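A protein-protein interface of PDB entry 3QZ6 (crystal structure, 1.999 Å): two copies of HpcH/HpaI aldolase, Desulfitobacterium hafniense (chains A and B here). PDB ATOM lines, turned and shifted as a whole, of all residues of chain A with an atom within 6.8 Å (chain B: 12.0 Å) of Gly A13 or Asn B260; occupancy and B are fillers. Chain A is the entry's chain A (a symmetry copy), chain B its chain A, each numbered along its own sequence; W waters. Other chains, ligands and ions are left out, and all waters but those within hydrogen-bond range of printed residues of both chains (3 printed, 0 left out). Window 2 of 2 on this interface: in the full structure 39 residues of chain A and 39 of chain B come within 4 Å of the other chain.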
ATOM      1  N   LYS A   7     -30.522 -28.587   6.401  1.00  0.00           N
ATOM      2  CA  LYS A   7     -31.983 -28.453   6.504  1.00  0.00           C
ATOM      3  C   LYS A   7     -32.440 -28.293   7.949  1.00  0.00           C
ATOM      4  O   LYS A   7     -33.450 -27.647   8.224  1.00  0.00           O
ATOM      5  CB  LYS A   7     -32.707 -29.632   5.855  1.00  0.00           C
ATOM      6  CG  LYS A   7     -32.522 -29.707   4.357  1.00  0.00           C
ATOM      7  CD  LYS A   7     -33.808 -29.452   3.611  1.00  0.00           C
ATOM      8  CE  LYS A   7     -34.917 -30.354   4.098  1.00  0.00           C
ATOM      9  NZ  LYS A   7     -35.991 -30.502   3.084  1.00  0.00           N
ATOM     10  N   LYS A   8     -31.691 -28.886   8.870  1.00  0.00           N
ATOM     11  CA  LYS A   8     -31.988 -28.758  10.290  1.00  0.00           C
ATOM     12  C   LYS A   8     -31.955 -27.281  10.700  1.00  0.00           C
ATOM     13  O   LYS A   8     -32.849 -26.791  11.383  1.00  0.00           O
ATOM     14  CB  LYS A   8     -30.970 -29.568  11.092  1.00  0.00           C
ATOM     15  CG  LYS A   8     -31.395 -29.951  12.488  1.00  0.00           C
ATOM     16  CD  LYS A   8     -30.418 -30.972  13.067  1.00  0.00           C
ATOM     17  CE  LYS A   8     -30.639 -31.197  14.562  1.00  0.00           C
ATOM     18  NZ  LYS A   8     -29.606 -32.108  15.146  1.00  0.00           N
ATOM     19  N   LYS A   9     -30.925 -26.567  10.266  1.00  0.00           N
ATOM     20  CA  LYS A   9     -30.826 -25.136  10.527  1.00  0.00           C
ATOM     21  C   LYS A   9     -31.953 -24.343   9.872  1.00  0.00           C
ATOM     22  O   LYS A   9     -32.563 -23.481  10.501  1.00  0.00           O
ATOM     23  CB  LYS A   9     -29.482 -24.608  10.032  1.00  0.00           C
ATOM     24  CG  LYS A   9     -28.298 -25.204  10.772  1.00  0.00           C
ATOM     25  CD  LYS A   9     -26.977 -24.801  10.128  1.00  0.00           C
ATOM     26  CE  LYS A   9     -25.805 -25.243  10.995  1.00  0.00           C
ATOM     27  NZ  LYS A   9     -24.512 -25.047  10.292  1.00  0.00           N
ATOM     28  N   LEU A  10     -32.224 -24.633   8.604  1.00  0.00           N
ATOM     29  CA  LEU A  10     -33.232 -23.901   7.858  1.00  0.00           C
ATOM     30  C   LEU A  10     -34.587 -24.134   8.489  1.00  0.00           C
ATOM     31  O   LEU A  10     -35.399 -23.216   8.619  1.00  0.00           O
ATOM     32  CB  LEU A  10     -33.267 -24.364   6.401  1.00  0.00           C
ATOM     33  CG  LEU A  10     -32.053 -23.994   5.556  1.00  0.00           C
ATOM     34  CD1 LEU A  10     -32.157 -24.625   4.177  1.00  0.00           C
ATOM     35  CD2 LEU A  10     -31.928 -22.482   5.461  1.00  0.00           C
ATOM     36  N   SER A  11     -34.820 -25.378   8.881  1.00  0.00           N
ATOM     37  CA  SER A  11     -36.088 -25.765   9.481  1.00  0.00           C
ATOM     38  C   SER A  11     -36.336 -25.016  10.792  1.00  0.00           C
ATOM     39  O   SER A  11     -37.480 -24.733  11.149  1.00  0.00           O
ATOM     40  CB  SER A  11     -36.112 -27.275   9.716  1.00  0.00           C
ATOM     41  OG  SER A  11     -37.301 -27.670  10.366  1.00  0.00           O
ATOM     42  N   ALA A  12     -35.262 -24.686  11.501  1.00  0.00           N
ATOM     43  CA  ALA A  12     -35.369 -23.957  12.762  1.00  0.00           C
ATOM     44  C   ALA A  12     -35.487 -22.451  12.541  1.00  0.00           C
ATOM     45  O   ALA A  12     -35.478 -21.669  13.494  1.00  0.00           O
ATOM     46  CB  ALA A  12     -34.180 -24.265  13.652  1.00  0.00           C
ATOM     47  N   GLY A  13     -35.588 -22.048  11.278  1.00  0.00           N
ATOM     48  CA  GLY A  13     -35.769 -20.649  10.931  1.00  0.00           C
ATOM     49  C   GLY A  13     -34.490 -19.835  10.896  1.00  0.00           C
ATOM     50  O   GLY A  13     -34.543 -18.611  10.803  1.00  0.00           O
ATOM     51  N   LYS A  14     -33.341 -20.505  10.954  1.00  0.00           N
ATOM     52  CA  LYS A  14     -32.054 -19.813  10.990  1.00  0.00           C
ATOM     53  C   LYS A  14     -31.643 -19.249   9.635  1.00  0.00           C
ATOM     54  O   LYS A  14     -31.973 -19.805   8.586  1.00  0.00           O
ATOM     55  CB  LYS A  14     -30.942 -20.753  11.458  1.00  0.00           C
ATOM     56  CG  LYS A  14     -31.053 -21.263  12.887  1.00  0.00           C
ATOM     57  CD  LYS A  14     -29.852 -22.158  13.183  1.00  0.00           C
ATOM     58  CE  LYS A  14     -29.879 -22.725  14.593  1.00  0.00           C
ATOM     59  NZ  LYS A  14     -29.853 -21.652  15.617  1.00  0.00           N
ATOM     60  N   SER A  15     -30.899 -18.152   9.671  1.00  0.00           N
ATOM     61  CA  SER A  15     -30.194 -17.664   8.499  1.00  0.00           C
ATOM     62  C   SER A  15     -28.878 -18.425   8.411  1.00  0.00           C
ATOM     63  O   SER A  15     -28.229 -18.651   9.423  1.00  0.00           O
ATOM     64  CB  SER A  15     -29.910 -16.171   8.638  1.00  0.00           C
ATOM     65  OG  SER A  15     -31.103 -15.453   8.903  1.00  0.00           O
ATOM     66  N   VAL A  16     -28.485 -18.842   7.212  1.00  0.00           N
ATOM     67  CA  VAL A  16     -27.231 -19.579   7.063  1.00  0.00           C
ATOM     68  C   VAL A  16     -26.378 -18.958   5.972  1.00  0.00           C
ATOM     69  O   VAL A  16     -26.894 -18.373   5.020  1.00  0.00           O
ATOM     70  CB  VAL A  16     -27.471 -21.075   6.775  1.00  0.00           C
ATOM     71  CG1 VAL A  16     -28.200 -21.721   7.948  1.00  0.00           C
ATOM     72  CG2 VAL A  16     -28.264 -21.254   5.482  1.00  0.00           C
ATOM     73  N   VAL A 226     -31.744 -10.217   3.346  1.00  0.00           N
ATOM     74  CA  VAL A 226     -32.038 -10.494   4.748  1.00  0.00           C
ATOM     75  C   VAL A 226     -33.333  -9.796   5.188  1.00  0.00           C
ATOM     76  O   VAL A 226     -34.172 -10.395   5.868  1.00  0.00           O
ATOM     77  CB  VAL A 226     -30.849 -10.106   5.651  1.00  0.00           C
ATOM     78  CG1 VAL A 226     -31.256 -10.107   7.122  1.00  0.00           C
ATOM     79  CG2 VAL A 226     -29.667 -11.068   5.404  1.00  0.00           C
ATOM     80  N   GLY A 229     -36.367 -11.846   4.277  1.00  0.00           N
ATOM     81  CA  GLY A 229     -36.570 -13.153   4.879  1.00  0.00           C
ATOM     82  C   GLY A 229     -35.791 -14.279   4.214  1.00  0.00           C
ATOM     83  O   GLY A 229     -36.074 -15.451   4.433  1.00  0.00           O
ATOM     84  N   GLN A 231     -33.195 -16.968   3.867  1.00  0.00           N
ATOM     85  CA  GLN A 231     -32.368 -17.727   4.809  1.00  0.00           C
ATOM     86  C   GLN A 231     -31.077 -18.274   4.186  1.00  0.00           C
ATOM     87  O   GLN A 231     -30.081 -18.483   4.893  1.00  0.00           O
ATOM     88  CB  GLN A 231     -33.147 -18.897   5.403  1.00  0.00           C
ATOM     89  CG  GLN A 231     -34.369 -18.537   6.216  1.00  0.00           C
ATOM     90  CD  GLN A 231     -35.115 -19.782   6.659  1.00  0.00           C
ATOM     91  OE1 GLN A 231     -36.148 -20.135   6.091  1.00  0.00           O
ATOM     92  NE2 GLN A 231     -34.574 -20.475   7.667  1.00  0.00           N
ATOM     93  N   VAL B 250     -18.418 -12.674   6.343  1.00  0.00           N
ATOM     94  CA  VAL B 250     -19.345 -13.476   7.129  1.00  0.00           C
ATOM     95  C   VAL B 250     -19.837 -12.687   8.344  1.00  0.00           C
ATOM     96  O   VAL B 250     -21.024 -12.675   8.653  1.00  0.00           O
ATOM     97  CB  VAL B 250     -18.693 -14.788   7.589  1.00  0.00           C
ATOM     98  CG1 VAL B 250     -19.554 -15.476   8.639  1.00  0.00           C
ATOM     99  CG2 VAL B 250     -18.458 -15.692   6.400  1.00  0.00           C
ATOM    100  N   LYS B 251     -18.917 -12.012   9.019  1.00  0.00           N
ATOM    101  CA  LYS B 251     -19.266 -11.245  10.207  1.00  0.00           C
ATOM    102  C   LYS B 251     -20.216 -10.096   9.852  1.00  0.00           C
ATOM    103  O   LYS B 251     -21.196  -9.846  10.553  1.00  0.00           O
ATOM    104  CB  LYS B 251     -17.994 -10.720  10.867  1.00  0.00           C
ATOM    105  CG  LYS B 251     -18.192  -9.904  12.135  1.00  0.00           C
ATOM    106  CD  LYS B 251     -16.824  -9.593  12.751  1.00  0.00           C
ATOM    107  CE  LYS B 251     -16.867  -8.406  13.706  1.00  0.00           C
ATOM    108  NZ  LYS B 251     -17.523  -8.777  14.975  1.00  0.00           N
ATOM    109  N   THR B 252     -19.921  -9.401   8.760  1.00  0.00           N
ATOM    110  CA  THR B 252     -20.791  -8.342   8.269  1.00  0.00           C
ATOM    111  C   THR B 252     -22.192  -8.889   8.031  1.00  0.00           C
ATOM    112  O   THR B 252     -23.180  -8.297   8.445  1.00  0.00           O
ATOM    113  CB  THR B 252     -20.227  -7.727   6.976  1.00  0.00           C
ATOM    114  OG1 THR B 252     -19.024  -7.000   7.276  1.00  0.00           O
ATOM    115  CG2 THR B 252     -21.233  -6.793   6.329  1.00  0.00           C
ATOM    116  N   ILE B 253     -22.278 -10.040   7.380  1.00  0.00           N
ATOM    117  CA  ILE B 253     -23.575 -10.646   7.100  1.00  0.00           C
ATOM    118  C   ILE B 253     -24.313 -11.002   8.391  1.00  0.00           C
ATOM    119  O   ILE B 253     -25.503 -10.714   8.545  1.00  0.00           O
ATOM    120  CB  ILE B 253     -23.420 -11.891   6.193  1.00  0.00           C
ATOM    121  CG1 ILE B 253     -22.922 -11.463   4.816  1.00  0.00           C
ATOM    122  CG2 ILE B 253     -24.755 -12.631   6.066  1.00  0.00           C
ATOM    123  CD1 ILE B 253     -22.411 -12.611   3.946  1.00  0.00           C
ATOM    124  N   LYS B 254     -23.605 -11.608   9.337  1.00  0.00           N
ATOM    125  CA  LYS B 254     -24.266 -12.059  10.556  1.00  0.00           C
ATOM    126  C   LYS B 254     -24.717 -10.885  11.418  1.00  0.00           C
ATOM    127  O   LYS B 254     -25.529 -11.051  12.329  1.00  0.00           O
ATOM    128  CB  LYS B 254     -23.375 -13.019  11.348  1.00  0.00           C
ATOM    129  CG  LYS B 254     -23.065 -14.295  10.577  1.00  0.00           C
ATOM    130  CD  LYS B 254     -22.603 -15.417  11.503  1.00  0.00           C
ATOM    131  CE  LYS B 254     -22.312 -16.679  10.701  1.00  0.00           C
ATOM    132  NZ  LYS B 254     -21.726 -17.759  11.539  1.00  0.00           N
ATOM    133  N   GLU B 255     -24.205  -9.698  11.110  1.00  0.00           N
ATOM    134  CA  GLU B 255     -24.581  -8.491  11.842  1.00  0.00           C
ATOM    135  C   GLU B 255     -25.710  -7.685  11.176  1.00  0.00           C
ATOM    136  O   GLU B 255     -26.125  -6.654  11.694  1.00  0.00           O
ATOM    137  CB  GLU B 255     -23.353  -7.615  12.074  1.00  0.00           C
ATOM    138  CG  GLU B 255     -22.349  -8.241  13.030  1.00  0.00           C
ATOM    139  CD  GLU B 255     -21.056  -7.451  13.146  1.00  0.00           C
ATOM    140  OE1 GLU B 255     -20.837  -6.528  12.329  1.00  0.00           O
ATOM    141  OE2 GLU B 255     -20.255  -7.765  14.056  1.00  0.00           O
ATOM    142  N   LEU B 256     -26.204  -8.153  10.033  1.00  0.00           N
ATOM    143  CA  LEU B 256     -27.294  -7.462   9.347  1.00  0.00           C
ATOM    144  C   LEU B 256     -28.582  -7.484  10.173  1.00  0.00           C
ATOM    145  O   LEU B 256     -28.881  -8.471  10.841  1.00  0.00           O
ATOM    146  CB  LEU B 256     -27.543  -8.082   7.972  1.00  0.00           C
ATOM    147  CG  LEU B 256     -26.402  -7.848   6.986  1.00  0.00           C
ATOM    148  CD1 LEU B 256     -26.530  -8.739   5.762  1.00  0.00           C
ATOM    149  CD2 LEU B 256     -26.327  -6.372   6.599  1.00  0.00           C
ATOM    150  N   PRO B 257     -29.353  -6.388  10.130  1.00  0.00           N
ATOM    151  CA  PRO B 257     -30.635  -6.389  10.843  1.00  0.00           C
ATOM    152  C   PRO B 257     -31.533  -7.459  10.245  1.00  0.00           C
ATOM    153  O   PRO B 257     -31.690  -7.495   9.025  1.00  0.00           O
ATOM    154  CB  PRO B 257     -31.218  -5.003  10.533  1.00  0.00           C
ATOM    155  CG  PRO B 257     -30.080  -4.186  10.032  1.00  0.00           C
ATOM    156  CD  PRO B 257     -29.135  -5.147   9.370  1.00  0.00           C
ATOM    157  N   GLY B 258     -32.106  -8.321  11.078  1.00  0.00           N
ATOM    158  CA  GLY B 258     -32.978  -9.372  10.581  1.00  0.00           C
ATOM    159  C   GLY B 258     -32.304 -10.730  10.473  1.00  0.00           C
ATOM    160  O   GLY B 258     -32.970 -11.736  10.244  1.00  0.00           O
ATOM    161  N   PHE B 259     -30.984 -10.775  10.631  1.00  0.00           N
ATOM    162  CA  PHE B 259     -30.290 -12.064  10.583  1.00  0.00           C
ATOM    163  C   PHE B 259     -30.737 -12.884  11.780  1.00  0.00           C
ATOM    164  O   PHE B 259     -30.812 -12.375  12.891  1.00  0.00           O
ATOM    165  CB  PHE B 259     -28.770 -11.876  10.606  1.00  0.00           C
ATOM    166  CG  PHE B 259     -27.989 -13.153  10.407  1.00  0.00           C
ATOM    167  CD1 PHE B 259     -27.610 -13.558   9.135  1.00  0.00           C
ATOM    168  CD2 PHE B 259     -27.624 -13.941  11.496  1.00  0.00           C
ATOM    169  CE1 PHE B 259     -26.873 -14.734   8.944  1.00  0.00           C
ATOM    170  CE2 PHE B 259     -26.895 -15.117  11.320  1.00  0.00           C
ATOM    171  CZ  PHE B 259     -26.521 -15.516  10.037  1.00  0.00           C
ATOM    172  N   ASN B 260     -31.055 -14.150  11.550  1.00  0.00           N
ATOM    173  CA  ASN B 260     -31.486 -15.020  12.635  1.00  0.00           C
ATOM    174  C   ASN B 260     -30.427 -16.074  12.961  1.00  0.00           C
ATOM    175  O   ASN B 260     -30.333 -17.096  12.285  1.00  0.00           O
ATOM    176  CB  ASN B 260     -32.832 -15.666  12.296  1.00  0.00           C
ATOM    177  CG  ASN B 260     -33.942 -14.638  12.142  1.00  0.00           C
ATOM    178  OD1 ASN B 260     -34.536 -14.498  11.073  1.00  0.00           O
ATOM    179  ND2 ASN B 260     -34.211 -13.901  13.208  1.00  0.00           N
ATOM    180  N   PRO B 261     -29.636 -15.822  14.016  1.00  0.00           N
ATOM    181  CA  PRO B 261     -28.487 -16.644  14.410  1.00  0.00           C
ATOM    182  C   PRO B 261     -28.899 -18.082  14.690  1.00  0.00           C
ATOM    183  O   PRO B 261     -29.985 -18.324  15.223  1.00  0.00           O
ATOM    184  CB  PRO B 261     -28.008 -15.989  15.713  1.00  0.00           C
ATOM    185  CG  PRO B 261     -28.678 -14.644  15.763  1.00  0.00           C
ATOM    186  CD  PRO B 261     -29.957 -14.793  15.019  1.00  0.00           C
ATOM    187  OXT PRO B 261     -28.155 -19.026  14.406  1.00  0.00           O
HETATM  188  O   HOH W   1     -33.903 -16.428   9.125  1.00  0.00           O
HETATM  189  O   HOH W   2     -33.961 -12.462   7.645  1.00  0.00           O
HETATM  190  O   HOH W   3     -27.375 -19.264  11.875  1.00  0.00           O
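The side-chain amide oxygen (OD1) of Asn B260 lies close to the backbone carbonyl oxygen (O) of Gly B258 (3.3 Å). O of Lys A9 sits at hydrogen-bond distance from N of Lys A14 (3.1 Å). The backbone carbonyl oxygen of Lys A14 is in hydrogen-bond range of the side-chain amide nitrogen of Gln A231, 2.8 Å away.
Asn B260 touches Gly A13 (CB to O, 3.7 Å). Lys A14 touches Asn B260 (CA to O, 3.5 Å). Ser A15 touches Phe B259. Val A226 touches Leu B256 (CG2 to CD1, 3.9 Å). CG1 of Val A226 touches O of Pro B257, 3.3 Å away. Val A226 touches Gly B258 (CG1 to C, 3.6 Å). Val A226 touches Phe B259 (CG1 to N, 3.6 Å).
The backbone NH (N) of Ser A15 sits at hydrogen-bond distance from the backbone carbonyl oxygen (O) of Asn B260 (2.9 Å). NZ of Lys A14 is in salt-bridge range of OXT of Pro B261, at 3.4 Å.
Leu A10 touches none of the printed residues of chain B. Ser A11 touches none of the printed residues of chain B. Of the printed residues of chain B, Ser A15 touches Phe B259 and Asn B260. No residue of chain B comes within 4 Å of Gly A229. Printed residues of chain A within 4 Å of Leu B256: Val A226 (3.9 Å). Of the printed residues of chain A, Gly B258 touches Val A226. Asn B260 touches just these residues of chain A: Gly A13, Lys A14 and Ser A15. Of the printed residues of chain A, Pro B261 touches Lys A14. The nearest residue of chain A that does not touch Asn B260 is Val A16 (5.7 Å).
Water W3 bridges OXT of Pro B261 and O of Ser A15. Water W2 lies within hydrogen-bond range of O of Val A226 and O of Gly B258. Water W1 lies within hydrogen-bond range of OD1 of Asn B260 (2.8 Å), O of Gly A13 (2.8 Å) and OG of Ser A15 (3.0 Å).
No position is printed for both chains. Of the 9 pairs that touch across the chains among the printed residues, none has its exchanged pair printed and touching as well.
Printed residues of chain B that touch a printed residue of chain A: Leu B256, Pro B257, Gly B258, Phe B259, Asn B260 and Pro B261. Hydrophobic or aromatic side chains of chain B that line the printed part of chain A: Leu B256 and Phe B259. Hydrophobic or aromatic side chains of chain A within 4 Å of the printed part of chain B: Val A226. Among the printed residues, no Asp or Glu carboxylate lies within 4 Å of a Lys or Arg side-chain nitrogen of the other chain.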
